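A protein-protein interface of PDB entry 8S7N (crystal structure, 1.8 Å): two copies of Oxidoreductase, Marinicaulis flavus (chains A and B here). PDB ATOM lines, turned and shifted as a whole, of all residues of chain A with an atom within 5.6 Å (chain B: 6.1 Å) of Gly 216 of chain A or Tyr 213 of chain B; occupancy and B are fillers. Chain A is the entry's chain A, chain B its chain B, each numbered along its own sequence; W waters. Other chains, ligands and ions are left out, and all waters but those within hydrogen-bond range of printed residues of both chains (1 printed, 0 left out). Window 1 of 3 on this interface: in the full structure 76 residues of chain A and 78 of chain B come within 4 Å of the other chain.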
ATOM      1  N   HIS A 163     -12.502  -6.956  -8.604  1.00  0.00           N
ATOM      2  CA  HIS A 163     -11.919  -6.208  -9.761  1.00  0.00           C
ATOM      3  C   HIS A 163     -11.054  -7.147 -10.616  1.00  0.00           C
ATOM      4  O   HIS A 163     -10.087  -6.682 -11.272  1.00  0.00           O
ATOM      5  CB  HIS A 163     -11.153  -4.939  -9.304  1.00  0.00           C
ATOM      6  CG  HIS A 163     -11.972  -3.977  -8.505  1.00  0.00           C
ATOM      7  ND1 HIS A 163     -11.368  -2.924  -7.812  1.00  0.00           N
ATOM      8  CD2 HIS A 163     -13.312  -3.876  -8.291  1.00  0.00           C
ATOM      9  CE1 HIS A 163     -12.323  -2.194  -7.258  1.00  0.00           C
ATOM     10  NE2 HIS A 163     -13.534  -2.729  -7.545  1.00  0.00           N
ATOM     11  N   PHE A 174     -15.629  -6.253 -13.553  1.00  0.00           N
ATOM     12  CA  PHE A 174     -16.512  -5.309 -12.849  1.00  0.00           C
ATOM     13  C   PHE A 174     -17.108  -4.302 -13.836  1.00  0.00           C
ATOM     14  O   PHE A 174     -18.280  -3.906 -13.601  1.00  0.00           O
ATOM     15  CB  PHE A 174     -15.884  -4.668 -11.627  1.00  0.00           C
ATOM     16  CG  PHE A 174     -16.959  -4.039 -10.765  1.00  0.00           C
ATOM     17  CD1 PHE A 174     -17.876  -4.813 -10.092  1.00  0.00           C
ATOM     18  CD2 PHE A 174     -17.128  -2.675 -10.732  1.00  0.00           C
ATOM     19  CE1 PHE A 174     -18.928  -4.245  -9.400  1.00  0.00           C
ATOM     20  CE2 PHE A 174     -18.159  -2.099 -10.013  1.00  0.00           C
ATOM     21  CZ  PHE A 174     -19.036  -2.874  -9.310  1.00  0.00           C
ATOM     22  N   GLN A 177     -20.434  -5.418 -15.175  1.00  0.00           N
ATOM     23  CA  GLN A 177     -21.515  -5.599 -14.173  1.00  0.00           C
ATOM     24  C   GLN A 177     -22.676  -4.643 -14.441  1.00  0.00           C
ATOM     25  O   GLN A 177     -22.490  -3.469 -14.851  1.00  0.00           O
ATOM     26  CB  GLN A 177     -20.962  -5.471 -12.754  1.00  0.00           C
ATOM     27  CG  GLN A 177     -22.033  -5.618 -11.672  1.00  0.00           C
ATOM     28  CD  GLN A 177     -22.630  -4.282 -11.273  1.00  0.00           C
ATOM     29  OE1 GLN A 177     -22.000  -3.229 -11.385  1.00  0.00           O
ATOM     30  NE2 GLN A 177     -23.833  -4.317 -10.736  1.00  0.00           N
ATOM     31  N   MET A 180     -27.266  -5.122  -9.212  1.00  0.00           N
ATOM     32  CA  MET A 180     -26.921  -6.117  -8.173  1.00  0.00           C
ATOM     33  C   MET A 180     -27.971  -6.066  -7.071  1.00  0.00           C
ATOM     34  O   MET A 180     -28.668  -5.035  -6.896  1.00  0.00           O
ATOM     35  CB  MET A 180     -25.518  -5.920  -7.603  1.00  0.00           C
ATOM     36  CG  MET A 180     -25.262  -4.564  -7.053  1.00  0.00           C
ATOM     37  SD  MET A 180     -23.701  -4.458  -6.135  1.00  0.00           S
ATOM     38  CE  MET A 180     -22.500  -4.732  -7.437  1.00  0.00           C
ATOM     39  N   TYR A 213     -24.831   6.484  -7.946  1.00  0.00           N
ATOM     40  CA  TYR A 213     -24.438   5.208  -8.590  1.00  0.00           C
ATOM     41  C   TYR A 213     -23.545   4.440  -7.617  1.00  0.00           C
ATOM     42  O   TYR A 213     -22.358   4.728  -7.507  1.00  0.00           O
ATOM     43  CB  TYR A 213     -23.839   5.460  -9.981  1.00  0.00           C
ATOM     44  CG  TYR A 213     -23.353   4.243 -10.726  1.00  0.00           C
ATOM     45  CD1 TYR A 213     -24.094   3.058 -10.762  1.00  0.00           C
ATOM     46  CD2 TYR A 213     -22.230   4.316 -11.522  1.00  0.00           C
ATOM     47  CE1 TYR A 213     -23.655   1.960 -11.486  1.00  0.00           C
ATOM     48  CE2 TYR A 213     -21.782   3.242 -12.266  1.00  0.00           C
ATOM     49  CZ  TYR A 213     -22.489   2.051 -12.229  1.00  0.00           C
ATOM     50  OH  TYR A 213     -22.030   1.019 -12.981  1.00  0.00           O
ATOM     51  N   VAL A 214     -24.118   3.444  -6.935  1.00  0.00           N
ATOM     52  CA  VAL A 214     -23.468   2.858  -5.730  1.00  0.00           C
ATOM     53  C   VAL A 214     -22.875   1.481  -6.009  1.00  0.00           C
ATOM     54  O   VAL A 214     -22.313   0.959  -5.061  1.00  0.00           O
ATOM     55  CB  VAL A 214     -24.462   2.801  -4.557  1.00  0.00           C
ATOM     56  CG1 VAL A 214     -24.902   4.205  -4.174  1.00  0.00           C
ATOM     57  CG2 VAL A 214     -25.664   1.903  -4.851  1.00  0.00           C
ATOM     58  N   ASP A 215     -23.138   0.845  -7.159  1.00  0.00           N
ATOM     59  CA  ASP A 215     -22.772  -0.578  -7.327  1.00  0.00           C
ATOM     60  C   ASP A 215     -21.290  -0.753  -6.954  1.00  0.00           C
ATOM     61  O   ASP A 215     -20.932  -1.721  -6.312  1.00  0.00           O
ATOM     62  CB  ASP A 215     -23.025  -1.071  -8.753  1.00  0.00           C
ATOM     63  CG  ASP A 215     -24.491  -1.003  -9.148  1.00  0.00           C
ATOM     64  OD1 ASP A 215     -25.061   0.093  -9.039  1.00  0.00           O
ATOM     65  OD2 ASP A 215     -25.041  -2.072  -9.468  1.00  0.00           O
ATOM     66  N   GLY A 216     -20.443   0.178  -7.380  1.00  0.00           N
ATOM     67  CA  GLY A 216     -18.998   0.156  -7.134  1.00  0.00           C
ATOM     68  C   GLY A 216     -18.601   0.059  -5.662  1.00  0.00           C
ATOM     69  O   GLY A 216     -17.510  -0.536  -5.385  1.00  0.00           O
ATOM     70  N   ILE A 217     -19.398   0.593  -4.749  1.00  0.00           N
ATOM     71  CA  ILE A 217     -19.005   0.628  -3.309  1.00  0.00           C
ATOM     72  C   ILE A 217     -19.095  -0.772  -2.733  1.00  0.00           C
ATOM     73  O   ILE A 217     -18.554  -0.966  -1.635  1.00  0.00           O
ATOM     74  CB  ILE A 217     -19.778   1.640  -2.447  1.00  0.00           C
ATOM     75  CG1 ILE A 217     -21.164   1.163  -2.032  1.00  0.00           C
ATOM     76  CG2 ILE A 217     -19.833   2.969  -3.144  1.00  0.00           C
ATOM     77  CD1 ILE A 217     -21.891   2.109  -1.107  1.00  0.00           C
ATOM     78  N   PHE A 218     -19.671  -1.736  -3.458  1.00  0.00           N
ATOM     79  CA  PHE A 218     -19.756  -3.112  -2.930  1.00  0.00           C
ATOM     80  C   PHE A 218     -18.666  -3.976  -3.557  1.00  0.00           C
ATOM     81  O   PHE A 218     -18.679  -5.157  -3.265  1.00  0.00           O
ATOM     82  CB  PHE A 218     -21.158  -3.676  -3.119  1.00  0.00           C
ATOM     83  CG  PHE A 218     -22.187  -2.828  -2.438  1.00  0.00           C
ATOM     84  CD1 PHE A 218     -22.275  -2.787  -1.048  1.00  0.00           C
ATOM     85  CD2 PHE A 218     -23.072  -2.050  -3.166  1.00  0.00           C
ATOM     86  CE1 PHE A 218     -23.210  -1.977  -0.428  1.00  0.00           C
ATOM     87  CE2 PHE A 218     -24.021  -1.264  -2.534  1.00  0.00           C
ATOM     88  CZ  PHE A 218     -24.082  -1.209  -1.164  1.00  0.00           C
ATOM     89  N   SER A 219     -17.774  -3.404  -4.378  1.00  0.00           N
ATOM     90  CA  SER A 219     -16.612  -4.122  -4.940  1.00  0.00           C
ATOM     91  C   SER A 219     -15.386  -3.788  -4.070  1.00  0.00           C
ATOM     92  O   SER A 219     -15.345  -2.673  -3.507  1.00  0.00           O
ATOM     93  CB  SER A 219     -16.436  -3.722  -6.407  1.00  0.00           C
ATOM     94  OG  SER A 219     -15.996  -2.367  -6.559  1.00  0.00           O
ATOM     95  N   GLN A 220     -14.498  -4.759  -3.883  1.00  0.00           N
ATOM     96  CA  GLN A 220     -13.325  -4.722  -2.949  1.00  0.00           C
ATOM     97  C   GLN A 220     -13.745  -4.085  -1.628  1.00  0.00           C
ATOM     98  O   GLN A 220     -13.081  -3.156  -1.135  1.00  0.00           O
ATOM     99  CB  GLN A 220     -12.134  -4.018  -3.617  1.00  0.00           C
ATOM    100  CG  GLN A 220     -11.485  -4.849  -4.712  1.00  0.00           C
ATOM    101  CD  GLN A 220     -10.078  -4.399  -5.020  1.00  0.00           C
ATOM    102  OE1 GLN A 220      -9.640  -3.354  -4.592  1.00  0.00           O
ATOM    103  NE2 GLN A 220      -9.349  -5.222  -5.755  1.00  0.00           N
ATOM    104  N   SER A 221     -14.852  -4.564  -1.065  1.00  0.00           N
ATOM    105  CA  SER A 221     -15.571  -3.822  -0.012  1.00  0.00           C
ATOM    106  C   SER A 221     -16.095  -4.758   1.088  1.00  0.00           C
ATOM    107  O   SER A 221     -16.241  -5.965   0.835  1.00  0.00           O
ATOM    108  CB  SER A 221     -16.720  -3.125  -0.636  1.00  0.00           C
ATOM    109  OG  SER A 221     -17.363  -2.344   0.313  1.00  0.00           O
ATOM    110  N   PHE B 174     -20.556   9.812 -18.067  1.00  0.00           N
ATOM    111  CA  PHE B 174     -20.064   9.351 -16.766  1.00  0.00           C
ATOM    112  C   PHE B 174     -19.229   8.060 -16.917  1.00  0.00           C
ATOM    113  O   PHE B 174     -18.277   7.916 -16.168  1.00  0.00           O
ATOM    114  CB  PHE B 174     -21.188   9.178 -15.751  1.00  0.00           C
ATOM    115  CG  PHE B 174     -20.572   9.023 -14.381  1.00  0.00           C
ATOM    116  CD1 PHE B 174     -19.910  10.101 -13.784  1.00  0.00           C
ATOM    117  CD2 PHE B 174     -20.561   7.812 -13.723  1.00  0.00           C
ATOM    118  CE1 PHE B 174     -19.246   9.971 -12.567  1.00  0.00           C
ATOM    119  CE2 PHE B 174     -19.909   7.690 -12.493  1.00  0.00           C
ATOM    120  CZ  PHE B 174     -19.259   8.761 -11.905  1.00  0.00           C
ATOM    121  N   GLN B 177     -15.564   8.691 -17.256  1.00  0.00           N
ATOM    122  CA  GLN B 177     -14.919   9.408 -16.121  1.00  0.00           C
ATOM    123  C   GLN B 177     -13.824   8.536 -15.546  1.00  0.00           C
ATOM    124  O   GLN B 177     -13.914   7.279 -15.546  1.00  0.00           O
ATOM    125  CB  GLN B 177     -15.962   9.857 -15.090  1.00  0.00           C
ATOM    126  CG  GLN B 177     -15.391  10.489 -13.841  1.00  0.00           C
ATOM    127  CD  GLN B 177     -15.108   9.496 -12.739  1.00  0.00           C
ATOM    128  OE1 GLN B 177     -15.701   8.430 -12.673  1.00  0.00           O
ATOM    129  NE2 GLN B 177     -14.136   9.804 -11.889  1.00  0.00           N
ATOM    130  N   LYS B 207      -9.373   3.458 -13.461  1.00  0.00           N
ATOM    131  CA  LYS B 207     -10.548   3.954 -12.690  1.00  0.00           C
ATOM    132  C   LYS B 207     -10.484   3.517 -11.213  1.00  0.00           C
ATOM    133  O   LYS B 207     -10.749   4.347 -10.357  1.00  0.00           O
ATOM    134  CB  LYS B 207     -11.850   3.439 -13.297  1.00  0.00           C
ATOM    135  CG  LYS B 207     -12.208   4.022 -14.629  1.00  0.00           C
ATOM    136  CD  LYS B 207     -13.334   3.223 -15.285  1.00  0.00           C
ATOM    137  CE  LYS B 207     -14.131   3.968 -16.337  1.00  0.00           C
ATOM    138  NZ  LYS B 207     -15.112   4.889 -15.715  1.00  0.00           N
ATOM    139  N   TYR B 208     -10.236   2.249 -10.880  1.00  0.00           N
ATOM    140  CA  TYR B 208     -10.642   1.728  -9.544  1.00  0.00           C
ATOM    141  C   TYR B 208      -9.725   2.223  -8.422  1.00  0.00           C
ATOM    142  O   TYR B 208     -10.183   2.465  -7.304  1.00  0.00           O
ATOM    143  CB  TYR B 208     -10.704   0.203  -9.523  1.00  0.00           C
ATOM    144  CG  TYR B 208     -11.621  -0.399 -10.559  1.00  0.00           C
ATOM    145  CD1 TYR B 208     -12.834   0.186 -10.886  1.00  0.00           C
ATOM    146  CD2 TYR B 208     -11.261  -1.552 -11.227  1.00  0.00           C
ATOM    147  CE1 TYR B 208     -13.677  -0.352 -11.854  1.00  0.00           C
ATOM    148  CE2 TYR B 208     -12.083  -2.112 -12.204  1.00  0.00           C
ATOM    149  CZ  TYR B 208     -13.316  -1.542 -12.482  1.00  0.00           C
ATOM    150  OH  TYR B 208     -14.092  -2.064 -13.460  1.00  0.00           O
ATOM    151  N   GLY B 211      -9.742  -0.842  -3.263  1.00  0.00           N
ATOM    152  CA  GLY B 211     -10.826  -0.738  -2.286  1.00  0.00           C
ATOM    153  C   GLY B 211     -12.139  -0.326  -2.939  1.00  0.00           C
ATOM    154  O   GLY B 211     -12.330  -0.430  -4.149  1.00  0.00           O
ATOM    155  N   PRO B 212     -13.116   0.116  -2.134  1.00  0.00           N
ATOM    156  CA  PRO B 212     -14.423   0.417  -2.678  1.00  0.00           C
ATOM    157  C   PRO B 212     -14.327   1.437  -3.822  1.00  0.00           C
ATOM    158  O   PRO B 212     -13.601   2.459  -3.715  1.00  0.00           O
ATOM    159  CB  PRO B 212     -15.224   0.906  -1.481  1.00  0.00           C
ATOM    160  CG  PRO B 212     -14.500   0.348  -0.280  1.00  0.00           C
ATOM    161  CD  PRO B 212     -13.048   0.238  -0.679  1.00  0.00           C
ATOM    162  N   TYR B 213     -15.120   1.201  -4.872  1.00  0.00           N
ATOM    163  CA  TYR B 213     -15.116   2.057  -6.079  1.00  0.00           C
ATOM    164  C   TYR B 213     -16.234   3.079  -5.885  1.00  0.00           C
ATOM    165  O   TYR B 213     -17.397   2.749  -6.106  1.00  0.00           O
ATOM    166  CB  TYR B 213     -15.299   1.199  -7.347  1.00  0.00           C
ATOM    167  CG  TYR B 213     -15.322   1.954  -8.649  1.00  0.00           C
ATOM    168  CD1 TYR B 213     -14.544   3.107  -8.838  1.00  0.00           C
ATOM    169  CD2 TYR B 213     -16.080   1.509  -9.716  1.00  0.00           C
ATOM    170  CE1 TYR B 213     -14.528   3.778 -10.060  1.00  0.00           C
ATOM    171  CE2 TYR B 213     -16.055   2.142 -10.949  1.00  0.00           C
ATOM    172  CZ  TYR B 213     -15.316   3.309 -11.100  1.00  0.00           C
ATOM    173  OH  TYR B 213     -15.332   3.940 -12.292  1.00  0.00           O
ATOM    174  N   VAL B 214     -15.902   4.282  -5.464  1.00  0.00           N
ATOM    175  CA  VAL B 214     -16.872   5.283  -4.935  1.00  0.00           C
ATOM    176  C   VAL B 214     -17.171   6.409  -5.907  1.00  0.00           C
ATOM    177  O   VAL B 214     -18.074   7.193  -5.559  1.00  0.00           O
ATOM    178  CB  VAL B 214     -16.416   5.872  -3.591  1.00  0.00           C
ATOM    179  CG1 VAL B 214     -16.245   4.785  -2.540  1.00  0.00           C
ATOM    180  CG2 VAL B 214     -15.159   6.723  -3.731  1.00  0.00           C
ATOM    181  N   ASP B 215     -16.522   6.511  -7.077  1.00  0.00           N
ATOM    182  CA  ASP B 215     -16.723   7.694  -7.941  1.00  0.00           C
ATOM    183  C   ASP B 215     -18.217   7.906  -8.193  1.00  0.00           C
ATOM    184  O   ASP B 215     -18.701   9.052  -8.162  1.00  0.00           O
ATOM    185  CB  ASP B 215     -15.922   7.557  -9.230  1.00  0.00           C
ATOM    186  CG  ASP B 215     -14.428   7.516  -8.962  1.00  0.00           C
ATOM    187  OD1 ASP B 215     -13.985   6.595  -8.306  1.00  0.00           O
ATOM    188  OD2 ASP B 215     -13.730   8.426  -9.430  1.00  0.00           O
ATOM    189  N   GLY B 216     -18.938   6.833  -8.515  1.00  0.00           N
ATOM    190  CA  GLY B 216     -20.339   6.954  -8.904  1.00  0.00           C
ATOM    191  C   GLY B 216     -21.209   7.531  -7.794  1.00  0.00           C
ATOM    192  O   GLY B 216     -22.298   8.052  -8.097  1.00  0.00           O
ATOM    193  N   ILE B 217     -20.809   7.480  -6.522  1.00  0.00           N
ATOM    194  CA  ILE B 217     -21.728   7.966  -5.458  1.00  0.00           C
ATOM    195  C   ILE B 217     -21.780   9.488  -5.504  1.00  0.00           C
ATOM    196  O   ILE B 217     -22.700  10.034  -4.890  1.00  0.00           O
ATOM    197  CB  ILE B 217     -21.411   7.418  -4.046  1.00  0.00           C
ATOM    198  CG1 ILE B 217     -20.239   8.131  -3.392  1.00  0.00           C
ATOM    199  CG2 ILE B 217     -21.209   5.902  -4.062  1.00  0.00           C
ATOM    200  CD1 ILE B 217     -20.022   7.775  -1.928  1.00  0.00           C
HETATM  201  O   HOH W   1     -19.926   3.970  -6.623  1.00  0.00           O
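Water W1 bridges O of Tyr 213 of chain A (2.7 Å) and O of Tyr 213 of chain B (2.9 Å).
Of the 13 printed residues of chain A, 8 touch a printed residue of chain B.
Hydrophobic or aromatic side chains of chain A that line the printed part of chain B: His 163, Phe 174, Tyr 213 and Ile 217.
Printed residues of chain B that touch a printed residue of chain A: Tyr 208, Gly 211, Pro 212, Tyr 213, Gly 216 and Ile 217.
Among the printed residues, 15 pairs touch across the chains.
Among the printed residues, no Asp or Glu carboxylate lies within 4 Å of a Lys or Arg side-chain nitrogen of the other chain.
O of Gly 216 of chain A is in hydrogen-bond range of OG of Ser 219 of chain A, 2.7 Å away.
O of Ile 217 of chain A sits at hydrogen-bond distance from OG of Ser 221 of chain A, at 2.7 Å.
A ring nitrogen (NE2) of His 163 of chain A is in hydrogen-bond range of the side-chain hydroxyl (OG) of Ser 219 of chain A, at 2.7 Å.
Among the printed residues, pairs that only touch across the chains: Ser 219 of chain A with Pro 212 of chain B, Ile 217 of chain A with Ile 217 of chain B, His 163 of chain A with Gly 211 of chain B, His 163 of chain A with Tyr 208 of chain B, Phe 174 of chain A with Tyr 208 of chain B, Ser 219 of chain A with Tyr 213 of chain B, Ser 219 of chain A with Gly 211 of chain B, Ile 217 of chain A with Pro 212 of chain B and Ser 221 of chain A with Pro 212 of chain B.
OE1 of Gln 220 of chain A is in hydrogen-bond range of N of Gly 211 of chain B, at 2.8 Å.
The backbone carbonyl oxygen (O) of Gly 216 of chain A sits at hydrogen-bond distance from the backbone NH (N) of Tyr 213 of chain B (3.0 Å).
The backbone carbonyl oxygen (O) of Gln 220 of chain A sits close to the backbone nitrogen (N) of Pro 212 of chain B (3.4 Å).
The backbone carbonyl oxygen (O) of Tyr 213 of chain A sits at hydrogen-bond distance from the backbone NH (N) of Ile 217 of chain B (3.3 Å).
O of Tyr 213 of chain B is in hydrogen-bond range of N of Ile 217 of chain A.
The backbone NH of Tyr 213 of chain A is in hydrogen-bond range of the backbone carbonyl oxygen of Gly 216 of chain B (3.0 Å).
Of the printed residues of chain B, His 163 of chain A touches Tyr 208 and Gly 211.
Asp 215 of chain A touches none of the printed residues of chain B.
Gly 216 of chain A touches one residue of chain B.
Of the printed residues of chain B, Ile 217 of chain A touches Pro 212, Tyr 213 and Ile 217.
Tyr 213 of chain A touches Gly 216 of chain B, and with the chains exchanged Gly 216 of chain A touches Tyr 213 of chain B.
Tyr 213 of chain A touches Ile 217 of chain B, and with the chains exchanged Ile 217 of chain A touches Tyr 213 of chain B.
Ile 217 of chain A touches its own counterpart, Ile 217 of chain B.
Positions printed for both chains: 174, 177, 213, 214, 215, 216 and 217.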
